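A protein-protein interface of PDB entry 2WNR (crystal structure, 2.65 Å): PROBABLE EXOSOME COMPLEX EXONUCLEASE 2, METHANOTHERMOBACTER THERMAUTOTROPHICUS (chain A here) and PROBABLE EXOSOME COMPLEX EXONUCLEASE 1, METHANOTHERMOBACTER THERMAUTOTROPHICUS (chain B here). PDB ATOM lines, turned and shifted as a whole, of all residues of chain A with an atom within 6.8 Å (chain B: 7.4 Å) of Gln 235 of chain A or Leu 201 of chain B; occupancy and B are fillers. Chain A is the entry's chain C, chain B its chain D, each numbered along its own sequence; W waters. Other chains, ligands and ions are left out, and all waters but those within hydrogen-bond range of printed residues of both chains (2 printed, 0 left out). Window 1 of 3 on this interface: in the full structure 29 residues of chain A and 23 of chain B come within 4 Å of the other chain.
Water W2 bridges OE1 of Glu 107 of chain B (2.6 Å) and OE2 of Glu 106 of chain A (2.8 Å). Water W1 lies within hydrogen-bond range of OE1 of Glu 107 of chain B, NZ of Lys 236 of chain A and O of Thr 199 of chain B.
Hydrophobic or aromatic side chains of chain B that line the printed part of chain A: Ile 104, Ile 198, Leu 201 and Phe 212. Hydrophobic or aromatic side chains of chain A within 4 Å of the printed part of chain B: Met 234, Leu 242 and Val 247. Among the printed residues, 21 pairs touch across the chains. Among the printed residues, Asp or Glu carboxylates within 4 Å of a Lys or Arg side-chain nitrogen of the other chain: Glu 106 of chain A with Lys 103 of chain B (3.7 Å) and Arg 113 of chain A with Glu 100 of chain B (2.9 Å).
Ala 233 of chain A touches Ser 203 of chain B (CA to O, 3.3 Å). Met 234 of chain A touches Leu 201 of chain B. O of Met 234 of chain A touches CA of Gln 202 of chain B, 3.3 Å away. Met 234 of chain A touches Phe 212 of chain B (SD to CZ, 3.3 Å). Ile 104 of chain B touches Gln 235 of chain A (CG2 to NE2, 3.8 Å). Lys 236 of chain A touches Ile 198 of chain B (CE to O, 3.9 Å). Glu 107 of chain B touches Gly 237 of chain A (OE1 to CA, 3.9 Å). CD1 of Ile 198 of chain B touches CG2 of Val 247 of chain A, at 3.7 Å. Val 247 of chain A touches Leu 201 of chain B (CG1 to CD2, 3.6 Å).
The backbone carbonyl oxygen (O) of Arg 220 of chain A lies within hydrogen-bond range of the backbone NH (N) of Gly 237 of chain A (2.7 Å). The backbone NH of Ser 222 of chain A is in hydrogen-bond range of the backbone carbonyl oxygen of Gln 235 of chain A, at 2.9 Å. NH1 of Arg 137 of chain B is in hydrogen-bond range of OE1 of Gln 202 of chain B (2.8 Å). The backbone NH (N) of Gln 202 of chain B lies within hydrogen-bond range of the backbone carbonyl oxygen (O) of Pro 188 of chain B (3.2 Å).
The side-chain carboxylate (OE1) of Glu 106 of chain A lies within salt-bridge range of the side-chain amino group (NZ) of Lys 103 of chain B (3.7 Å). NH2 of Arg 113 of chain A lies within salt-bridge range of OE2 of Glu 100 of chain B (2.9 Å). NH2 of Arg 113 of chain A sits close to NE2 of Gln 202 of chain B, 3.5 Å away. The backbone carbonyl oxygen (O) of Ser 203 of chain B sits at hydrogen-bond distance from the backbone NH (N) of Met 234 of chain A. OE2 of Glu 100 of chain B lies within hydrogen-bond range of NE2 of Gln 235 of chain A (3.1 Å). OE1 of Gln 235 of chain A is in hydrogen-bond range of NE2 of Gln 202 of chain B, 2.9 Å away. The side-chain amino group (NZ) of Lys 236 of chain A is in hydrogen-bond range of the backbone carbonyl oxygen (O) of Thr 199 of chain B, at 2.9 Å. The backbone NH (N) of Lys 236 of chain A is in hydrogen-bond range of the backbone carbonyl oxygen (O) of Leu 201 of chain B (2.9 Å). The backbone NH of Ile 198 of chain B is in hydrogen-bond range of the backbone carbonyl oxygen of Leu 242 of chain A (2.6 Å).
Printed residues of chain B within 4 Å of Glu 106 of chain A: Lys 103. Of the printed residues of chain B, Arg 113 of chain A touches Glu 100 (2.9 Å), Gln 202 (3.5 Å) and Ser 203 (3.6 Å). Gly 224 of chain A touches none of the printed residues of chain B. Of the printed residues of chain B, Met 234 of chain A touches Leu 201 (3.8 Å), Gln 202 (3.3 Å), Ser 203 (3.0 Å) and Phe 212 (3.3 Å). Of chain B, only Glu 100, Ile 104, Leu 201 and Gln 202 come within 4 Å of Gln 235 of chain A. Printed residues of chain B within 4 Å of Val 247 of chain A: Ile 198, Leu 201 and Phe 212. Pro 188 of chain B touches none of the printed residues of chain A. Of chain A, only Met 234, Gln 235, Lys 236 and Val 247 come within 4 Å of Leu 201 of chain B. The nearest residue of chain B that does not touch Gln 235 of chain A is Ser 203 of chain B (5.1 Å). The nearest residue of chain A that does not touch Leu 201 of chain B is Ile 221 of chain A (4.2 Å). The nearest printed residue of chain A that does not touch Thr 199 of chain B is Leu 242 of chain A (5.0 Å).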
ATOM      1  N   GLU A 106      -6.649  -4.007 -22.601  1.00  0.00           N
ATOM      2  CA  GLU A 106      -5.525  -4.875 -22.314  1.00  0.00           C
ATOM      3  C   GLU A 106      -5.103  -4.688 -20.867  1.00  0.00           C
ATOM      4  O   GLU A 106      -5.014  -5.649 -20.108  1.00  0.00           O
ATOM      5  CB  GLU A 106      -4.351  -4.607 -23.249  1.00  0.00           C
ATOM      6  CG  GLU A 106      -3.187  -5.546 -23.003  1.00  0.00           C
ATOM      7  CD  GLU A 106      -1.897  -5.040 -23.593  1.00  0.00           C
ATOM      8  OE1 GLU A 106      -1.800  -3.815 -23.834  1.00  0.00           O
ATOM      9  OE2 GLU A 106      -0.971  -5.860 -23.810  1.00  0.00           O
ATOM     10  N   VAL A 110      -5.237  -7.681 -18.147  1.00  0.00           N
ATOM     11  CA  VAL A 110      -3.986  -8.136 -17.561  1.00  0.00           C
ATOM     12  C   VAL A 110      -4.038  -8.045 -16.029  1.00  0.00           C
ATOM     13  O   VAL A 110      -3.619  -8.974 -15.335  1.00  0.00           O
ATOM     14  CB  VAL A 110      -2.762  -7.415 -18.178  1.00  0.00           C
ATOM     15  CG1 VAL A 110      -1.508  -7.686 -17.372  1.00  0.00           C
ATOM     16  CG2 VAL A 110      -2.561  -7.891 -19.591  1.00  0.00           C
ATOM     17  N   ARG A 113      -6.329 -10.691 -14.797  1.00  0.00           N
ATOM     18  CA  ARG A 113      -5.675 -11.992 -14.900  1.00  0.00           C
ATOM     19  C   ARG A 113      -4.831 -12.247 -13.658  1.00  0.00           C
ATOM     20  O   ARG A 113      -4.947 -13.297 -13.014  1.00  0.00           O
ATOM     21  CB  ARG A 113      -4.805 -12.038 -16.151  1.00  0.00           C
ATOM     22  CG  ARG A 113      -4.329 -13.424 -16.542  1.00  0.00           C
ATOM     23  CD  ARG A 113      -3.508 -13.362 -17.811  1.00  0.00           C
ATOM     24  NE  ARG A 113      -4.238 -12.677 -18.871  1.00  0.00           N
ATOM     25  CZ  ARG A 113      -3.666 -12.031 -19.879  1.00  0.00           C
ATOM     26  NH1 ARG A 113      -2.337 -11.986 -19.981  1.00  0.00           N
ATOM     27  NH2 ARG A 113      -4.428 -11.420 -20.782  1.00  0.00           N
ATOM     28  N   PHE A 151       0.721  -1.017 -15.833  1.00  0.00           N
ATOM     29  CA  PHE A 151       0.447  -2.369 -15.312  1.00  0.00           C
ATOM     30  C   PHE A 151       0.875  -2.561 -13.863  1.00  0.00           C
ATOM     31  O   PHE A 151       0.076  -2.994 -13.031  1.00  0.00           O
ATOM     32  CB  PHE A 151       1.085  -3.448 -16.190  1.00  0.00           C
ATOM     33  CG  PHE A 151       0.707  -3.354 -17.630  1.00  0.00           C
ATOM     34  CD1 PHE A 151      -0.389  -4.046 -18.112  1.00  0.00           C
ATOM     35  CD2 PHE A 151       1.461  -2.571 -18.519  1.00  0.00           C
ATOM     36  CE1 PHE A 151      -0.750  -3.956 -19.454  1.00  0.00           C
ATOM     37  CE2 PHE A 151       1.115  -2.478 -19.863  1.00  0.00           C
ATOM     38  CZ  PHE A 151       0.008  -3.167 -20.333  1.00  0.00           C
ATOM     39  N   MET A 195       3.008  -7.439  -9.755  1.00  0.00           N
ATOM     40  CA  MET A 195       3.492  -7.476 -11.128  1.00  0.00           C
ATOM     41  C   MET A 195       4.714  -6.595 -11.400  1.00  0.00           C
ATOM     42  O   MET A 195       4.825  -5.480 -10.901  1.00  0.00           O
ATOM     43  CB  MET A 195       2.348  -7.106 -12.070  1.00  0.00           C
ATOM     44  CG  MET A 195       2.696  -7.187 -13.548  1.00  0.00           C
ATOM     45  SD  MET A 195       1.242  -7.265 -14.606  1.00  0.00           S
ATOM     46  CE  MET A 195       0.588  -8.888 -14.227  1.00  0.00           C
ATOM     47  N   THR A 197       6.816  -5.100 -14.764  1.00  0.00           N
ATOM     48  CA  THR A 197       6.856  -4.892 -16.207  1.00  0.00           C
ATOM     49  C   THR A 197       8.247  -4.442 -16.609  1.00  0.00           C
ATOM     50  O   THR A 197       8.809  -3.538 -16.003  1.00  0.00           O
ATOM     51  CB  THR A 197       5.831  -3.830 -16.667  1.00  0.00           C
ATOM     52  OG1 THR A 197       4.510  -4.270 -16.345  1.00  0.00           O
ATOM     53  CG2 THR A 197       5.927  -3.578 -18.170  1.00  0.00           C
ATOM     54  N   ARG A 220       7.784  -5.057 -24.562  1.00  0.00           N
ATOM     55  CA  ARG A 220       7.658  -5.041 -23.115  1.00  0.00           C
ATOM     56  C   ARG A 220       7.114  -6.384 -22.650  1.00  0.00           C
ATOM     57  O   ARG A 220       6.461  -7.090 -23.422  1.00  0.00           O
ATOM     58  CB  ARG A 220       6.703  -3.922 -22.683  1.00  0.00           C
ATOM     59  CG  ARG A 220       5.310  -4.093 -23.237  1.00  0.00           C
ATOM     60  CD  ARG A 220       4.334  -3.032 -22.804  1.00  0.00           C
ATOM     61  NE  ARG A 220       3.044  -3.665 -22.690  1.00  0.00           N
ATOM     62  CZ  ARG A 220       1.991  -3.538 -23.485  1.00  0.00           C
ATOM     63  NH1 ARG A 220       1.942  -2.719 -24.524  1.00  0.00           N
ATOM     64  NH2 ARG A 220       0.941  -4.261 -23.181  1.00  0.00           N
ATOM     65  N   ILE A 221       7.389  -6.734 -21.396  1.00  0.00           N
ATOM     66  CA  ILE A 221       6.815  -7.943 -20.800  1.00  0.00           C
ATOM     67  C   ILE A 221       6.409  -7.747 -19.338  1.00  0.00           C
ATOM     68  O   ILE A 221       7.199  -7.306 -18.507  1.00  0.00           O
ATOM     69  CB  ILE A 221       7.741  -9.188 -20.968  1.00  0.00           C
ATOM     70  CG1 ILE A 221       7.058 -10.439 -20.394  1.00  0.00           C
ATOM     71  CG2 ILE A 221       9.129  -8.936 -20.356  1.00  0.00           C
ATOM     72  CD1 ILE A 221       7.664 -11.749 -20.830  1.00  0.00           C
ATOM     73  N   SER A 222       5.163  -8.073 -19.034  1.00  0.00           N
ATOM     74  CA  SER A 222       4.660  -7.956 -17.673  1.00  0.00           C
ATOM     75  C   SER A 222       4.550  -9.336 -17.060  1.00  0.00           C
ATOM     76  O   SER A 222       4.039 -10.258 -17.695  1.00  0.00           O
ATOM     77  CB  SER A 222       3.311  -7.264 -17.668  1.00  0.00           C
ATOM     78  OG  SER A 222       3.427  -5.968 -18.210  1.00  0.00           O
ATOM     79  N   ILE A 223       5.053  -9.479 -15.836  1.00  0.00           N
ATOM     80  CA  ILE A 223       5.024 -10.766 -15.155  1.00  0.00           C
ATOM     81  C   ILE A 223       4.413 -10.658 -13.763  1.00  0.00           C
ATOM     82  O   ILE A 223       4.898  -9.905 -12.919  1.00  0.00           O
ATOM     83  CB  ILE A 223       6.415 -11.414 -15.090  1.00  0.00           C
ATOM     84  CG1 ILE A 223       6.978 -11.579 -16.499  1.00  0.00           C
ATOM     85  CG2 ILE A 223       6.336 -12.778 -14.397  1.00  0.00           C
ATOM     86  CD1 ILE A 223       8.460 -11.861 -16.539  1.00  0.00           C
ATOM     87  N   GLY A 224       3.332 -11.408 -13.547  1.00  0.00           N
ATOM     88  CA  GLY A 224       2.682 -11.482 -12.247  1.00  0.00           C
ATOM     89  C   GLY A 224       3.162 -12.682 -11.456  1.00  0.00           C
ATOM     90  O   GLY A 224       2.960 -13.820 -11.864  1.00  0.00           O
ATOM     91  N   ALA A 233       0.553 -14.596 -14.078  1.00  0.00           N
ATOM     92  CA  ALA A 233       0.187 -13.829 -15.273  1.00  0.00           C
ATOM     93  C   ALA A 233       1.406 -13.358 -16.056  1.00  0.00           C
ATOM     94  O   ALA A 233       2.422 -12.969 -15.468  1.00  0.00           O
ATOM     95  CB  ALA A 233      -0.701 -12.641 -14.906  1.00  0.00           C
ATOM     96  N   MET A 234       1.298 -13.396 -17.382  1.00  0.00           N
ATOM     97  CA  MET A 234       2.352 -12.895 -18.252  1.00  0.00           C
ATOM     98  C   MET A 234       1.772 -12.238 -19.495  1.00  0.00           C
ATOM     99  O   MET A 234       0.774 -12.711 -20.043  1.00  0.00           O
ATOM    100  CB  MET A 234       3.308 -14.019 -18.637  1.00  0.00           C
ATOM    101  CG  MET A 234       4.569 -13.531 -19.325  1.00  0.00           C
ATOM    102  SD  MET A 234       5.736 -14.846 -19.675  1.00  0.00           S
ATOM    103  CE  MET A 234       6.299 -15.219 -18.015  1.00  0.00           C
ATOM    104  N   GLN A 235       2.392 -11.144 -19.934  1.00  0.00           N
ATOM    105  CA  GLN A 235       1.912 -10.409 -21.098  1.00  0.00           C
ATOM    106  C   GLN A 235       3.034  -9.697 -21.840  1.00  0.00           C
ATOM    107  O   GLN A 235       3.573  -8.694 -21.367  1.00  0.00           O
ATOM    108  CB  GLN A 235       0.833  -9.404 -20.690  1.00  0.00           C
ATOM    109  CG  GLN A 235       0.192  -8.649 -21.850  1.00  0.00           C
ATOM    110  CD  GLN A 235      -0.974  -9.395 -22.481  1.00  0.00           C
ATOM    111  OE1 GLN A 235      -1.246 -10.547 -22.146  1.00  0.00           O
ATOM    112  NE2 GLN A 235      -1.677  -8.733 -23.401  1.00  0.00           N
ATOM    113  N   LYS A 236       3.377 -10.230 -23.008  1.00  0.00           N
ATOM    114  CA  LYS A 236       4.294  -9.571 -23.921  1.00  0.00           C
ATOM    115  C   LYS A 236       3.528  -8.488 -24.665  1.00  0.00           C
ATOM    116  O   LYS A 236       2.424  -8.728 -25.140  1.00  0.00           O
ATOM    117  CB  LYS A 236       4.883 -10.585 -24.908  1.00  0.00           C
ATOM    118  CG  LYS A 236       5.975 -10.034 -25.834  1.00  0.00           C
ATOM    119  CD  LYS A 236       5.428  -9.655 -27.197  1.00  0.00           C
ATOM    120  CE  LYS A 236       6.473  -8.964 -28.050  1.00  0.00           C
ATOM    121  NZ  LYS A 236       5.925  -8.556 -29.377  1.00  0.00           N
ATOM    122  N   GLY A 237       4.120  -7.302 -24.767  1.00  0.00           N
ATOM    123  CA  GLY A 237       3.520  -6.200 -25.514  1.00  0.00           C
ATOM    124  C   GLY A 237       4.524  -5.561 -26.446  1.00  0.00           C
ATOM    125  O   GLY A 237       5.706  -5.898 -26.407  1.00  0.00           O
ATOM    126  N   LEU A 242      10.869 -10.374 -28.598  1.00  0.00           N
ATOM    127  CA  LEU A 242      11.717 -10.715 -27.456  1.00  0.00           C
ATOM    128  C   LEU A 242      12.492 -11.991 -27.771  1.00  0.00           C
ATOM    129  O   LEU A 242      12.080 -12.786 -28.614  1.00  0.00           O
ATOM    130  CB  LEU A 242      10.856 -10.955 -26.213  1.00  0.00           C
ATOM    131  CG  LEU A 242      10.667  -9.888 -25.134  1.00  0.00           C
ATOM    132  CD1 LEU A 242      10.608  -8.491 -25.699  1.00  0.00           C
ATOM    133  CD2 LEU A 242       9.413 -10.203 -24.343  1.00  0.00           C
ATOM    134  N   VAL A 247      13.068 -13.199 -21.996  1.00  0.00           N
ATOM    135  CA  VAL A 247      11.899 -13.653 -21.253  1.00  0.00           C
ATOM    136  C   VAL A 247      12.302 -14.303 -19.938  1.00  0.00           C
ATOM    137  O   VAL A 247      11.748 -13.970 -18.888  1.00  0.00           O
ATOM    138  CB  VAL A 247      11.041 -14.620 -22.090  1.00  0.00           C
ATOM    139  CG1 VAL A 247       9.934 -15.241 -21.241  1.00  0.00           C
ATOM    140  CG2 VAL A 247      10.468 -13.895 -23.295  1.00  0.00           C
ATOM    141  N   GLU B 100      -8.639  -7.673 -27.267  1.00  0.00           N
ATOM    142  CA  GLU B 100      -7.270  -7.936 -26.801  1.00  0.00           C
ATOM    143  C   GLU B 100      -6.523  -8.792 -27.801  1.00  0.00           C
ATOM    144  O   GLU B 100      -5.372  -8.514 -28.113  1.00  0.00           O
ATOM    145  CB  GLU B 100      -7.248  -8.611 -25.428  1.00  0.00           C
ATOM    146  CG  GLU B 100      -5.842  -8.664 -24.826  1.00  0.00           C
ATOM    147  CD  GLU B 100      -5.675  -9.691 -23.705  1.00  0.00           C
ATOM    148  OE1 GLU B 100      -6.687 -10.258 -23.232  1.00  0.00           O
ATOM    149  OE2 GLU B 100      -4.515  -9.927 -23.291  1.00  0.00           O
ATOM    150  N   LYS B 103      -5.451  -6.882 -30.751  1.00  0.00           N
ATOM    151  CA  LYS B 103      -4.320  -6.020 -30.394  1.00  0.00           C
ATOM    152  C   LYS B 103      -2.981  -6.763 -30.465  1.00  0.00           C
ATOM    153  O   LYS B 103      -2.051  -6.315 -31.138  1.00  0.00           O
ATOM    154  CB  LYS B 103      -4.527  -5.412 -29.008  1.00  0.00           C
ATOM    155  CG  LYS B 103      -3.582  -4.280 -28.673  1.00  0.00           C
ATOM    156  CD  LYS B 103      -3.562  -4.025 -27.176  1.00  0.00           C
ATOM    157  CE  LYS B 103      -2.976  -2.667 -26.841  1.00  0.00           C
ATOM    158  NZ  LYS B 103      -1.603  -2.522 -27.322  1.00  0.00           N
ATOM    159  N   ILE B 104      -2.899  -7.905 -29.789  1.00  0.00           N
ATOM    160  CA  ILE B 104      -1.632  -8.645 -29.709  1.00  0.00           C
ATOM    161  C   ILE B 104      -1.278  -9.430 -30.984  1.00  0.00           C
ATOM    162  O   ILE B 104      -0.105  -9.751 -31.206  1.00  0.00           O
ATOM    163  CB  ILE B 104      -1.543  -9.550 -28.442  1.00  0.00           C
ATOM    164  CG1 ILE B 104      -2.574 -10.672 -28.492  1.00  0.00           C
ATOM    165  CG2 ILE B 104      -1.691  -8.714 -27.182  1.00  0.00           C
ATOM    166  CD1 ILE B 104      -2.574 -11.568 -27.262  1.00  0.00           C
ATOM    167  N   GLU B 107       0.393  -7.052 -33.286  1.00  0.00           N
ATOM    168  CA  GLU B 107       1.752  -6.929 -32.784  1.00  0.00           C
ATOM    169  C   GLU B 107       2.531  -8.187 -33.095  1.00  0.00           C
ATOM    170  O   GLU B 107       3.715  -8.113 -33.382  1.00  0.00           O
ATOM    171  CB  GLU B 107       1.766  -6.646 -31.279  1.00  0.00           C
ATOM    172  CG  GLU B 107       1.484  -5.182 -30.895  1.00  0.00           C
ATOM    173  CD  GLU B 107       1.374  -4.952 -29.379  1.00  0.00           C
ATOM    174  OE1 GLU B 107       1.216  -5.929 -28.611  1.00  0.00           O
ATOM    175  OE2 GLU B 107       1.442  -3.777 -28.957  1.00  0.00           O
ATOM    176  N   ALA B 108       1.864  -9.339 -33.061  1.00  0.00           N
ATOM    177  CA  ALA B 108       2.530 -10.615 -33.346  1.00  0.00           C
ATOM    178  C   ALA B 108       3.029 -10.722 -34.799  1.00  0.00           C
ATOM    179  O   ALA B 108       4.135 -11.203 -35.044  1.00  0.00           O
ATOM    180  CB  ALA B 108       1.624 -11.789 -32.996  1.00  0.00           C
ATOM    181  N   ARG B 137      -6.307 -18.053 -30.774  1.00  0.00           N
ATOM    182  CA  ARG B 137      -5.469 -16.878 -31.000  1.00  0.00           C
ATOM    183  C   ARG B 137      -4.169 -17.271 -31.702  1.00  0.00           C
ATOM    184  O   ARG B 137      -3.711 -16.570 -32.601  1.00  0.00           O
ATOM    185  CB  ARG B 137      -5.225 -16.087 -29.705  1.00  0.00           C
ATOM    186  CG  ARG B 137      -4.237 -16.710 -28.733  1.00  0.00           C
ATOM    187  CD  ARG B 137      -4.290 -16.039 -27.398  1.00  0.00           C
ATOM    188  NE  ARG B 137      -5.595 -16.223 -26.784  1.00  0.00           N
ATOM    189  CZ  ARG B 137      -6.082 -15.432 -25.835  1.00  0.00           C
ATOM    190  NH1 ARG B 137      -5.362 -14.401 -25.394  1.00  0.00           N
ATOM    191  NH2 ARG B 137      -7.294 -15.665 -25.332  1.00  0.00           N
ATOM    192  N   VAL B 187       0.050 -21.275 -21.929  1.00  0.00           N
ATOM    193  CA  VAL B 187       1.154 -20.406 -22.345  1.00  0.00           C
ATOM    194  C   VAL B 187       1.245 -20.312 -23.877  1.00  0.00           C
ATOM    195  O   VAL B 187       2.088 -20.988 -24.493  1.00  0.00           O
ATOM    196  CB  VAL B 187       2.509 -20.890 -21.764  1.00  0.00           C
ATOM    197  CG1 VAL B 187       3.619 -19.875 -22.027  1.00  0.00           C
ATOM    198  CG2 VAL B 187       2.391 -21.141 -20.285  1.00  0.00           C
ATOM    199  N   PRO B 188       0.369 -19.480 -24.494  1.00  0.00           N
ATOM    200  CA  PRO B 188       0.426 -19.237 -25.941  1.00  0.00           C
ATOM    201  C   PRO B 188       1.716 -18.512 -26.345  1.00  0.00           C
ATOM    202  O   PRO B 188       2.124 -17.559 -25.675  1.00  0.00           O
ATOM    203  CB  PRO B 188      -0.797 -18.343 -26.194  1.00  0.00           C
ATOM    204  CG  PRO B 188      -1.082 -17.716 -24.890  1.00  0.00           C
ATOM    205  CD  PRO B 188      -0.734 -18.734 -23.862  1.00  0.00           C
ATOM    206  N   VAL B 189       2.346 -18.982 -27.421  1.00  0.00           N
ATOM    207  CA  VAL B 189       3.575 -18.391 -27.952  1.00  0.00           C
ATOM    208  C   VAL B 189       3.465 -18.247 -29.465  1.00  0.00           C
ATOM    209  O   VAL B 189       2.933 -19.127 -30.138  1.00  0.00           O
ATOM    210  CB  VAL B 189       4.822 -19.266 -27.627  1.00  0.00           C
ATOM    211  CG1 VAL B 189       6.111 -18.623 -28.152  1.00  0.00           C
ATOM    212  CG2 VAL B 189       4.946 -19.498 -26.139  1.00  0.00           C
ATOM    213  N   ALA B 190       3.953 -17.131 -29.992  1.00  0.00           N
ATOM    214  CA  ALA B 190       4.147 -16.988 -31.431  1.00  0.00           C
ATOM    215  C   ALA B 190       5.568 -16.545 -31.670  1.00  0.00           C
ATOM    216  O   ALA B 190       6.065 -15.674 -30.949  1.00  0.00           O
ATOM    217  CB  ALA B 190       3.191 -15.997 -32.013  1.00  0.00           C
ATOM    218  N   ILE B 198      10.537 -14.199 -30.108  1.00  0.00           N
ATOM    219  CA  ILE B 198       9.222 -14.328 -29.469  1.00  0.00           C
ATOM    220  C   ILE B 198       8.383 -13.090 -29.736  1.00  0.00           C
ATOM    221  O   ILE B 198       8.687 -11.989 -29.266  1.00  0.00           O
ATOM    222  CB  ILE B 198       9.334 -14.616 -27.958  1.00  0.00           C
ATOM    223  CG1 ILE B 198      10.145 -15.899 -27.735  1.00  0.00           C
ATOM    224  CG2 ILE B 198       7.944 -14.737 -27.338  1.00  0.00           C
ATOM    225  CD1 ILE B 198      10.640 -16.091 -26.323  1.00  0.00           C
ATOM    226  N   THR B 199       7.316 -13.303 -30.495  1.00  0.00           N
ATOM    227  CA  THR B 199       6.533 -12.229 -31.078  1.00  0.00           C
ATOM    228  C   THR B 199       5.194 -12.059 -30.338  1.00  0.00           C
ATOM    229  O   THR B 199       4.602 -10.977 -30.333  1.00  0.00           O
ATOM    230  CB  THR B 199       6.379 -12.483 -32.602  1.00  0.00           C
ATOM    231  OG1 THR B 199       6.500 -11.254 -33.319  1.00  0.00           O
ATOM    232  CG2 THR B 199       5.080 -13.169 -32.940  1.00  0.00           C
ATOM    233  N   LEU B 200       4.736 -13.144 -29.718  1.00  0.00           N
ATOM    234  CA  LEU B 200       3.611 -13.131 -28.796  1.00  0.00           C
ATOM    235  C   LEU B 200       3.979 -14.042 -27.644  1.00  0.00           C
ATOM    236  O   LEU B 200       4.703 -15.031 -27.836  1.00  0.00           O
ATOM    237  CB  LEU B 200       2.339 -13.650 -29.469  1.00  0.00           C
ATOM    238  CG  LEU B 200       1.033 -13.720 -28.661  1.00  0.00           C
ATOM    239  CD1 LEU B 200      -0.149 -13.438 -29.553  1.00  0.00           C
ATOM    240  CD2 LEU B 200       0.842 -15.056 -27.940  1.00  0.00           C
ATOM    241  N   LEU B 201       3.474 -13.711 -26.455  1.00  0.00           N
ATOM    242  CA  LEU B 201       3.654 -14.540 -25.265  1.00  0.00           C
ATOM    243  C   LEU B 201       2.702 -14.145 -24.138  1.00  0.00           C
ATOM    244  O   LEU B 201       2.651 -12.985 -23.718  1.00  0.00           O
ATOM    245  CB  LEU B 201       5.109 -14.497 -24.781  1.00  0.00           C
ATOM    246  CG  LEU B 201       5.489 -15.326 -23.554  1.00  0.00           C
ATOM    247  CD1 LEU B 201       5.206 -16.801 -23.748  1.00  0.00           C
ATOM    248  CD2 LEU B 201       6.950 -15.110 -23.256  1.00  0.00           C
ATOM    249  N   GLN B 202       1.941 -15.121 -23.658  1.00  0.00           N
ATOM    250  CA  GLN B 202       1.062 -14.912 -22.507  1.00  0.00           C
ATOM    251  C   GLN B 202       1.158 -16.103 -21.565  1.00  0.00           C
ATOM    252  O   GLN B 202       1.710 -17.141 -21.920  1.00  0.00           O
ATOM    253  CB  GLN B 202      -0.392 -14.720 -22.933  1.00  0.00           C
ATOM    254  CG  GLN B 202      -0.652 -13.516 -23.797  1.00  0.00           C
ATOM    255  CD  GLN B 202      -2.108 -13.416 -24.198  1.00  0.00           C
ATOM    256  OE1 GLN B 202      -2.626 -14.269 -24.918  1.00  0.00           O
ATOM    257  NE2 GLN B 202      -2.787 -12.378 -23.715  1.00  0.00           N
ATOM    258  N   SER B 203       0.628 -15.938 -20.363  1.00  0.00           N
ATOM    259  CA  SER B 203       0.545 -17.014 -19.400  1.00  0.00           C
ATOM    260  C   SER B 203      -0.550 -16.689 -18.411  1.00  0.00           C
ATOM    261  O   SER B 203      -0.679 -15.550 -17.967  1.00  0.00           O
ATOM    262  CB  SER B 203       1.866 -17.178 -18.655  1.00  0.00           C
ATOM    263  OG  SER B 203       1.666 -17.775 -17.386  1.00  0.00           O
ATOM    264  N   PHE B 212       7.375 -23.046 -16.313  1.00  0.00           N
ATOM    265  CA  PHE B 212       7.185 -22.105 -17.399  1.00  0.00           C
ATOM    266  C   PHE B 212       8.243 -22.298 -18.477  1.00  0.00           C
ATOM    267  O   PHE B 212       7.918 -22.385 -19.656  1.00  0.00           O
ATOM    268  CB  PHE B 212       7.190 -20.661 -16.891  1.00  0.00           C
ATOM    269  CG  PHE B 212       7.208 -19.645 -17.994  1.00  0.00           C
ATOM    270  CD1 PHE B 212       6.029 -19.259 -18.620  1.00  0.00           C
ATOM    271  CD2 PHE B 212       8.412 -19.096 -18.431  1.00  0.00           C
ATOM    272  CE1 PHE B 212       6.049 -18.338 -19.650  1.00  0.00           C
ATOM    273  CE2 PHE B 212       8.438 -18.172 -19.469  1.00  0.00           C
ATOM    274  CZ  PHE B 212       7.258 -17.795 -20.077  1.00  0.00           C
ATOM    275  N   ALA B 215       7.321 -25.146 -20.637  1.00  0.00           N
ATOM    276  CA  ALA B 215       6.134 -24.893 -21.468  1.00  0.00           C
ATOM    277  C   ALA B 215       6.398 -23.968 -22.649  1.00  0.00           C
ATOM    278  O   ALA B 215       5.912 -24.212 -23.757  1.00  0.00           O
ATOM    279  CB  ALA B 215       4.989 -24.369 -20.626  1.00  0.00           C
ATOM    280  N   LEU B 216       7.164 -22.909 -22.410  1.00  0.00           N
ATOM    281  CA  LEU B 216       7.668 -22.057 -23.480  1.00  0.00           C
ATOM    282  C   LEU B 216       8.450 -22.876 -24.524  1.00  0.00           C
ATOM    283  O   LEU B 216       8.123 -22.821 -25.716  1.00  0.00           O
ATOM    284  CB  LEU B 216       8.537 -20.932 -22.903  1.00  0.00           C
ATOM    285  CG  LEU B 216       9.451 -20.114 -23.821  1.00  0.00           C
ATOM    286  CD1 LEU B 216       8.648 -19.184 -24.702  1.00  0.00           C
ATOM    287  CD2 LEU B 216      10.460 -19.325 -23.018  1.00  0.00           C
ATOM    288  N   ALA B 219       6.294 -25.187 -26.499  1.00  0.00           N
ATOM    289  CA  ALA B 219       5.477 -24.428 -27.431  1.00  0.00           C
ATOM    290  C   ALA B 219       6.293 -24.060 -28.666  1.00  0.00           C
ATOM    291  O   ALA B 219       5.805 -24.162 -29.793  1.00  0.00           O
ATOM    292  CB  ALA B 219       4.927 -23.175 -26.751  1.00  0.00           C
HETATM  293  O   HOH W   1       2.795  -8.411 -28.884  1.00  0.00           O
HETATM  294  O   HOH W   2      -0.029  -5.540 -26.379  1.00  0.00           O
